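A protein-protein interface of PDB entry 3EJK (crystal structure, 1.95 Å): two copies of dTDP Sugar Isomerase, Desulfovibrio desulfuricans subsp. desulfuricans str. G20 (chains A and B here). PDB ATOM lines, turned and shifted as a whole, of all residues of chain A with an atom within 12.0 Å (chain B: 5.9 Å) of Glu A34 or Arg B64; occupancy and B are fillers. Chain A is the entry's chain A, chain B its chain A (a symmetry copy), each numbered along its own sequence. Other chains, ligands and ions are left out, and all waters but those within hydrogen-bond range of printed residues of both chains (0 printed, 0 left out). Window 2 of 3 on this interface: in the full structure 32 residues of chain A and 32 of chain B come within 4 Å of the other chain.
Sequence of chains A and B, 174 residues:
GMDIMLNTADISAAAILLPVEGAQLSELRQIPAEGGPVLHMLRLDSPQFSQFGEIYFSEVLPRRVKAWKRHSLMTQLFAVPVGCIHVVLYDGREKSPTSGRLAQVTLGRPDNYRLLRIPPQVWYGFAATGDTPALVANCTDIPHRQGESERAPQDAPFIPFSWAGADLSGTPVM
The backbone carbonyl oxygen of Gly A35 sits at hydrogen-bond distance from the backbone NH of Leu B61 (2.8 Å). The backbone carbonyl oxygen (O) of Gly A36 lies within hydrogen-bond range of the side-chain amino group (NZ) of Lys B66 (2.7 Å). NH2 of Arg B64 is in salt-bridge range of OE1 of Glu A34 (3.1 Å).
O of Phe B126 sits at hydrogen-bond distance from N of Lys B66, 2.7 Å away. The backbone NH (N) of Ala B128 is in hydrogen-bond range of the backbone carbonyl oxygen (O) of Arg B64 (3.2 Å).
O of Glu A34 touches CE of Lys B66, 3.6 Å away. O of Gly A35 touches CA of Val B60 (3.4 Å). Arg B64 touches Gly A35 (NH2 to N, 3.6 Å). C of Gly A35 touches CE of Lys B66 (3.99 Å).
Glu A34 touches two residues of chain B. Of the printed residues of chain B, Gly A35 touches Val B60, Leu B61, Arg B64 and Lys B66. Printed residues of chain B within 4 Å of Gly A36: Lys B66. Pro A37 touches none of the printed residues of chain B. Leu A39 touches none of the printed residues of chain B. Val B60 touches one residue of chain A. Of chain A, only Gly A35 (2.8 Å) comes within 4 Å of Leu B61. No residue of chain A comes within 4 Å of Pro B62. Arg B64 touches just these residues of chain A: Glu A34 and Gly A35. Printed residues of chain A within 4 Å of Lys B66: Glu A34 (3.6 Å), Gly A35 (3.99 Å) and Gly A36 (2.7 Å). No residue of chain A comes within 4 Å of Ala B127. The nearest residue of chain B that does not touch Glu A34 is Val B65 (4.8 Å). The nearest residue of chain A that does not touch Arg B64 is Gly A36 (5.8 Å). The nearest printed residue of chain B that does not touch Gly A35 is Val B65 (5.2 Å).
Printed residues of chain B that touch a printed residue of chain A: Val B60, Leu B61, Arg B64 and Lys B66. Hydrophobic or aromatic side chains of chain B within 4 Å of the printed part of chain A: Leu B61. Printed residues of chain A that touch a printed residue of chain B: Glu A34, Gly A35 and Gly A36. Among the printed residues, 7 pairs touch across the chains. Among the printed residues, Asp or Glu carboxylates within 4 Å of a Lys or Arg side-chain nitrogen of the other chain: Glu A34 with Arg B64 (3.1 Å).
No position is printed for both chains.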
ATOM      1  N   GLN A  30      27.375   4.395 -18.183  1.00  0.00           N
ATOM      2  CA  GLN A  30      26.069   3.929 -18.680  1.00  0.00           C
ATOM      3  C   GLN A  30      25.020   4.796 -17.987  1.00  0.00           C
ATOM      4  O   GLN A  30      24.887   4.777 -16.762  1.00  0.00           O
ATOM      5  CB  GLN A  30      25.828   2.443 -18.378  1.00  0.00           C
ATOM      6  CG  GLN A  30      26.942   1.507 -18.869  1.00  0.00           C
ATOM      7  CD  GLN A  30      26.735   0.049 -18.464  1.00  0.00           C
ATOM      8  OE1 GLN A  30      25.717  -0.571 -18.778  1.00  0.00           O
ATOM      9  NE2 GLN A  30      27.711  -0.503 -17.769  1.00  0.00           N
ATOM     10  N   ILE A  31      24.299   5.592 -18.763  1.00  0.00           N
ATOM     11  CA  ILE A  31      23.295   6.473 -18.198  1.00  0.00           C
ATOM     12  C   ILE A  31      21.931   5.759 -18.197  1.00  0.00           C
ATOM     13  O   ILE A  31      21.421   5.374 -19.245  1.00  0.00           O
ATOM     14  CB  ILE A  31      23.176   7.823 -18.949  1.00  0.00           C
ATOM     15  CG1 ILE A  31      24.551   8.456 -19.180  1.00  0.00           C
ATOM     16  CG2 ILE A  31      22.251   8.784 -18.199  1.00  0.00           C
ATOM     17  CD1 ILE A  31      25.409   8.489 -17.956  1.00  0.00           C
ATOM     18  N   PRO A  32      21.349   5.553 -17.015  1.00  0.00           N
ATOM     19  CA  PRO A  32      20.044   4.918 -17.054  1.00  0.00           C
ATOM     20  C   PRO A  32      19.010   5.831 -17.658  1.00  0.00           C
ATOM     21  O   PRO A  32      19.071   7.040 -17.476  1.00  0.00           O
ATOM     22  CB  PRO A  32      19.716   4.668 -15.574  1.00  0.00           C
ATOM     23  CG  PRO A  32      21.014   4.863 -14.831  1.00  0.00           C
ATOM     24  CD  PRO A  32      21.814   5.812 -15.642  1.00  0.00           C
ATOM     25  N   ALA A  33      18.091   5.228 -18.402  1.00  0.00           N
ATOM     26  CA  ALA A  33      16.998   5.955 -19.051  1.00  0.00           C
ATOM     27  C   ALA A  33      15.848   5.044 -19.472  1.00  0.00           C
ATOM     28  O   ALA A  33      16.037   3.868 -19.780  1.00  0.00           O
ATOM     29  CB  ALA A  33      17.537   6.700 -20.255  1.00  0.00           C
ATOM     30  N   GLU A  34      14.649   5.600 -19.482  1.00  0.00           N
ATOM     31  CA  GLU A  34      13.466   4.812 -19.880  1.00  0.00           C
ATOM     32  C   GLU A  34      13.597   4.354 -21.318  1.00  0.00           C
ATOM     33  O   GLU A  34      13.908   5.118 -22.205  1.00  0.00           O
ATOM     34  CB  GLU A  34      12.178   5.572 -19.649  1.00  0.00           C
ATOM     35  CG  GLU A  34      11.710   5.541 -18.192  1.00  0.00           C
ATOM     36  CD  GLU A  34      11.062   4.190 -17.773  1.00  0.00           C
ATOM     37  OE1 GLU A  34      11.331   3.149 -18.382  1.00  0.00           O
ATOM     38  OE2 GLU A  34      10.281   4.174 -16.819  1.00  0.00           O
ATOM     39  N   GLY A  35      13.429   3.064 -21.509  1.00  0.00           N
ATOM     40  CA  GLY A  35      13.469   2.474 -22.840  1.00  0.00           C
ATOM     41  C   GLY A  35      14.778   1.792 -23.035  1.00  0.00           C
ATOM     42  O   GLY A  35      14.934   0.943 -23.899  1.00  0.00           O
ATOM     43  N   GLY A  36      15.724   2.179 -22.207  1.00  0.00           N
ATOM     44  CA  GLY A  36      17.059   1.581 -22.263  1.00  0.00           C
ATOM     45  C   GLY A  36      18.174   2.575 -22.036  1.00  0.00           C
ATOM     46  O   GLY A  36      18.018   3.756 -22.285  1.00  0.00           O
ATOM     47  N   PRO A  37      19.337   2.086 -21.606  1.00  0.00           N
ATOM     48  CA  PRO A  37      20.367   3.040 -21.266  1.00  0.00           C
ATOM     49  C   PRO A  37      21.121   3.637 -22.412  1.00  0.00           C
ATOM     50  O   PRO A  37      21.165   3.103 -23.520  1.00  0.00           O
ATOM     51  CB  PRO A  37      21.329   2.201 -20.408  1.00  0.00           C
ATOM     52  CG  PRO A  37      21.196   0.821 -20.967  1.00  0.00           C
ATOM     53  CD  PRO A  37      19.720   0.707 -21.252  1.00  0.00           C
ATOM     54  N   VAL A  38      21.697   4.780 -22.086  1.00  0.00           N
ATOM     55  CA  VAL A  38      22.623   5.494 -22.967  1.00  0.00           C
ATOM     56  C   VAL A  38      24.021   5.055 -22.552  1.00  0.00           C
ATOM     57  O   VAL A  38      24.388   5.064 -21.362  1.00  0.00           O
ATOM     58  CB  VAL A  38      22.466   7.013 -22.851  1.00  0.00           C
ATOM     59  CG1 VAL A  38      23.590   7.732 -23.546  1.00  0.00           C
ATOM     60  CG2 VAL A  38      21.089   7.450 -23.389  1.00  0.00           C
ATOM     61  N   LEU A  39      24.777   4.635 -23.547  1.00  0.00           N
ATOM     62  CA  LEU A  39      26.120   4.137 -23.340  1.00  0.00           C
ATOM     63  C   LEU A  39      27.152   5.037 -23.978  1.00  0.00           C
ATOM     64  O   LEU A  39      27.180   5.217 -25.194  1.00  0.00           O
ATOM     65  CB  LEU A  39      26.235   2.737 -23.921  1.00  0.00           C
ATOM     66  CG  LEU A  39      25.113   1.776 -23.528  1.00  0.00           C
ATOM     67  CD1 LEU A  39      25.207   0.485 -24.313  1.00  0.00           C
ATOM     68  CD2 LEU A  39      25.178   1.539 -22.017  1.00  0.00           C
ATOM     69  N   ARG A 109      28.898  -5.455 -21.153  1.00  0.00           N
ATOM     70  CA  ARG A 109      27.936  -5.176 -20.094  1.00  0.00           C
ATOM     71  C   ARG A 109      27.543  -6.445 -19.362  1.00  0.00           C
ATOM     72  O   ARG A 109      27.534  -7.515 -19.946  1.00  0.00           O
ATOM     73  CB  ARG A 109      26.687  -4.497 -20.669  1.00  0.00           C
ATOM     74  CG  ARG A 109      26.970  -3.118 -21.184  1.00  0.00           C
ATOM     75  CD  ARG A 109      25.655  -2.395 -21.429  1.00  0.00           C
ATOM     76  NE  ARG A 109      25.108  -2.762 -22.706  1.00  0.00           N
ATOM     77  CZ  ARG A 109      23.825  -2.755 -23.023  1.00  0.00           C
ATOM     78  NH1 ARG A 109      22.895  -2.463 -22.133  1.00  0.00           N
ATOM     79  NH2 ARG A 109      23.488  -3.088 -24.244  1.00  0.00           N
ATOM     80  N   VAL B  60      17.538   0.578 -27.121  1.00  0.00           N
ATOM     81  CA  VAL B  60      16.091   0.688 -27.126  1.00  0.00           C
ATOM     82  C   VAL B  60      15.522  -0.714 -27.063  1.00  0.00           C
ATOM     83  O   VAL B  60      15.717  -1.512 -27.977  1.00  0.00           O
ATOM     84  CB  VAL B  60      15.541   1.437 -28.360  1.00  0.00           C
ATOM     85  CG1 VAL B  60      14.034   1.678 -28.210  1.00  0.00           C
ATOM     86  CG2 VAL B  60      16.260   2.777 -28.525  1.00  0.00           C
ATOM     87  N   LEU B  61      14.859  -1.016 -25.952  1.00  0.00           N
ATOM     88  CA  LEU B  61      14.239  -2.333 -25.773  1.00  0.00           C
ATOM     89  C   LEU B  61      13.050  -2.452 -26.731  1.00  0.00           C
ATOM     90  O   LEU B  61      12.451  -1.441 -27.122  1.00  0.00           O
ATOM     91  CB  LEU B  61      13.801  -2.560 -24.331  1.00  0.00           C
ATOM     92  CG  LEU B  61      14.935  -2.574 -23.319  1.00  0.00           C
ATOM     93  CD1 LEU B  61      14.366  -2.871 -21.944  1.00  0.00           C
ATOM     94  CD2 LEU B  61      15.968  -3.606 -23.690  1.00  0.00           C
ATOM     95  N   PRO B  62      12.677  -3.686 -27.083  1.00  0.00           N
ATOM     96  CA  PRO B  62      11.604  -3.849 -28.072  1.00  0.00           C
ATOM     97  C   PRO B  62      10.314  -3.198 -27.676  1.00  0.00           C
ATOM     98  O   PRO B  62       9.840  -3.352 -26.561  1.00  0.00           O
ATOM     99  CB  PRO B  62      11.429  -5.376 -28.189  1.00  0.00           C
ATOM    100  CG  PRO B  62      12.176  -5.978 -27.053  1.00  0.00           C
ATOM    101  CD  PRO B  62      13.229  -4.977 -26.631  1.00  0.00           C
ATOM    102  N   ARG B  63       9.788  -2.478 -28.650  1.00  0.00           N
ATOM    103  CA  ARG B  63       8.493  -1.773 -28.603  1.00  0.00           C
ATOM    104  C   ARG B  63       8.540  -0.548 -27.735  1.00  0.00           C
ATOM    105  O   ARG B  63       7.524   0.087 -27.532  1.00  0.00           O
ATOM    106  CB  ARG B  63       7.333  -2.664 -28.150  1.00  0.00           C
ATOM    107  CG  ARG B  63       7.219  -3.993 -28.863  1.00  0.00           C
ATOM    108  CD  ARG B  63       7.088  -3.874 -30.338  1.00  0.00           C
ATOM    109  NE  ARG B  63       7.100  -5.202 -30.941  1.00  0.00           N
ATOM    110  CZ  ARG B  63       6.026  -5.862 -31.360  1.00  0.00           C
ATOM    111  NH1 ARG B  63       4.830  -5.308 -31.298  1.00  0.00           N
ATOM    112  NH2 ARG B  63       6.162  -7.067 -31.886  1.00  0.00           N
ATOM    113  N   ARG B  64       9.728  -0.237 -27.236  1.00  0.00           N
ATOM    114  CA  ARG B  64       9.964   0.967 -26.440  1.00  0.00           C
ATOM    115  C   ARG B  64      10.238   2.192 -27.329  1.00  0.00           C
ATOM    116  O   ARG B  64      10.858   2.125 -28.406  1.00  0.00           O
ATOM    117  CB  ARG B  64      11.093   0.749 -25.429  1.00  0.00           C
ATOM    118  CG  ARG B  64      10.792  -0.359 -24.401  1.00  0.00           C
ATOM    119  CD  ARG B  64       9.516  -0.142 -23.654  1.00  0.00           C
ATOM    120  NE  ARG B  64       9.537   1.110 -22.903  1.00  0.00           N
ATOM    121  CZ  ARG B  64       9.965   1.226 -21.658  1.00  0.00           C
ATOM    122  NH1 ARG B  64      10.398   0.166 -21.017  1.00  0.00           N
ATOM    123  NH2 ARG B  64       9.951   2.401 -21.055  1.00  0.00           N
ATOM    124  N   VAL B  65       9.746   3.314 -26.837  1.00  0.00           N
ATOM    125  CA  VAL B  65       9.838   4.612 -27.532  1.00  0.00           C
ATOM    126  C   VAL B  65      10.704   5.638 -26.812  1.00  0.00           C
ATOM    127  O   VAL B  65      10.626   5.796 -25.593  1.00  0.00           O
ATOM    128  CB  VAL B  65       8.432   5.225 -27.656  1.00  0.00           C
ATOM    129  CG1 VAL B  65       8.476   6.613 -28.307  1.00  0.00           C
ATOM    130  CG2 VAL B  65       7.494   4.274 -28.418  1.00  0.00           C
ATOM    131  N   LYS B  66      11.538   6.320 -27.584  1.00  0.00           N
ATOM    132  CA  LYS B  66      12.325   7.449 -27.075  1.00  0.00           C
ATOM    133  C   LYS B  66      12.006   8.675 -27.910  1.00  0.00           C
ATOM    134  O   LYS B  66      12.507   8.855 -29.021  1.00  0.00           O
ATOM    135  CB  LYS B  66      13.826   7.171 -27.090  1.00  0.00           C
ATOM    136  CG  LYS B  66      14.253   6.060 -26.140  1.00  0.00           C
ATOM    137  CD  LYS B  66      15.773   5.952 -26.075  1.00  0.00           C
ATOM    138  CE  LYS B  66      16.213   4.959 -25.001  1.00  0.00           C
ATOM    139  NZ  LYS B  66      17.663   5.089 -24.657  1.00  0.00           N
ATOM    140  N   PHE B 126      12.201   7.938 -31.780  1.00  0.00           N
ATOM    141  CA  PHE B 126      12.412   6.613 -32.364  1.00  0.00           C
ATOM    142  C   PHE B 126      11.999   5.505 -31.419  1.00  0.00           C
ATOM    143  O   PHE B 126      11.924   5.693 -30.202  1.00  0.00           O
ATOM    144  CB  PHE B 126      13.863   6.434 -32.841  1.00  0.00           C
ATOM    145  CG  PHE B 126      14.906   6.723 -31.787  1.00  0.00           C
ATOM    146  CD1 PHE B 126      15.322   5.746 -30.918  1.00  0.00           C
ATOM    147  CD2 PHE B 126      15.473   7.984 -31.678  1.00  0.00           C
ATOM    148  CE1 PHE B 126      16.293   6.003 -29.962  1.00  0.00           C
ATOM    149  CE2 PHE B 126      16.425   8.253 -30.726  1.00  0.00           C
ATOM    150  CZ  PHE B 126      16.837   7.258 -29.856  1.00  0.00           C
ATOM    151  N   ALA B 127      11.697   4.367 -32.023  1.00  0.00           N
ATOM    152  CA  ALA B 127      11.274   3.171 -31.305  1.00  0.00           C
ATOM    153  C   ALA B 127      11.788   1.894 -31.944  1.00  0.00           C
ATOM    154  O   ALA B 127      11.908   1.792 -33.150  1.00  0.00           O
ATOM    155  CB  ALA B 127       9.747   3.123 -31.209  1.00  0.00           C
ATOM    156  N   ALA B 128      12.059   0.921 -31.083  1.00  0.00           N
ATOM    157  CA  ALA B 128      12.518  -0.396 -31.508  1.00  0.00           C
ATOM    158  C   ALA B 128      11.337  -1.262 -31.906  1.00  0.00           C
ATOM    159  O   ALA B 128      10.359  -1.385 -31.180  1.00  0.00           O
ATOM    160  CB  ALA B 128      13.334  -1.097 -30.385  1.00  0.00           C
ATOM    161  N   LEU B 168       4.812  -1.221 -34.503  1.00  0.00           N
ATOM    162  CA  LEU B 168       6.180  -1.541 -34.146  1.00  0.00           C
ATOM    163  C   LEU B 168       6.421  -3.038 -34.225  1.00  0.00           C
ATOM    164  O   LEU B 168       7.328  -3.571 -33.599  1.00  0.00           O
ATOM    165  CB  LEU B 168       6.518  -1.006 -32.750  1.00  0.00           C
ATOM    166  CG  LEU B 168       6.318   0.513 -32.550  1.00  0.00           C
ATOM    167  CD1 LEU B 168       6.734   0.932 -31.149  1.00  0.00           C
ATOM    168  CD2 LEU B 168       7.077   1.296 -33.595  1.00  0.00           C
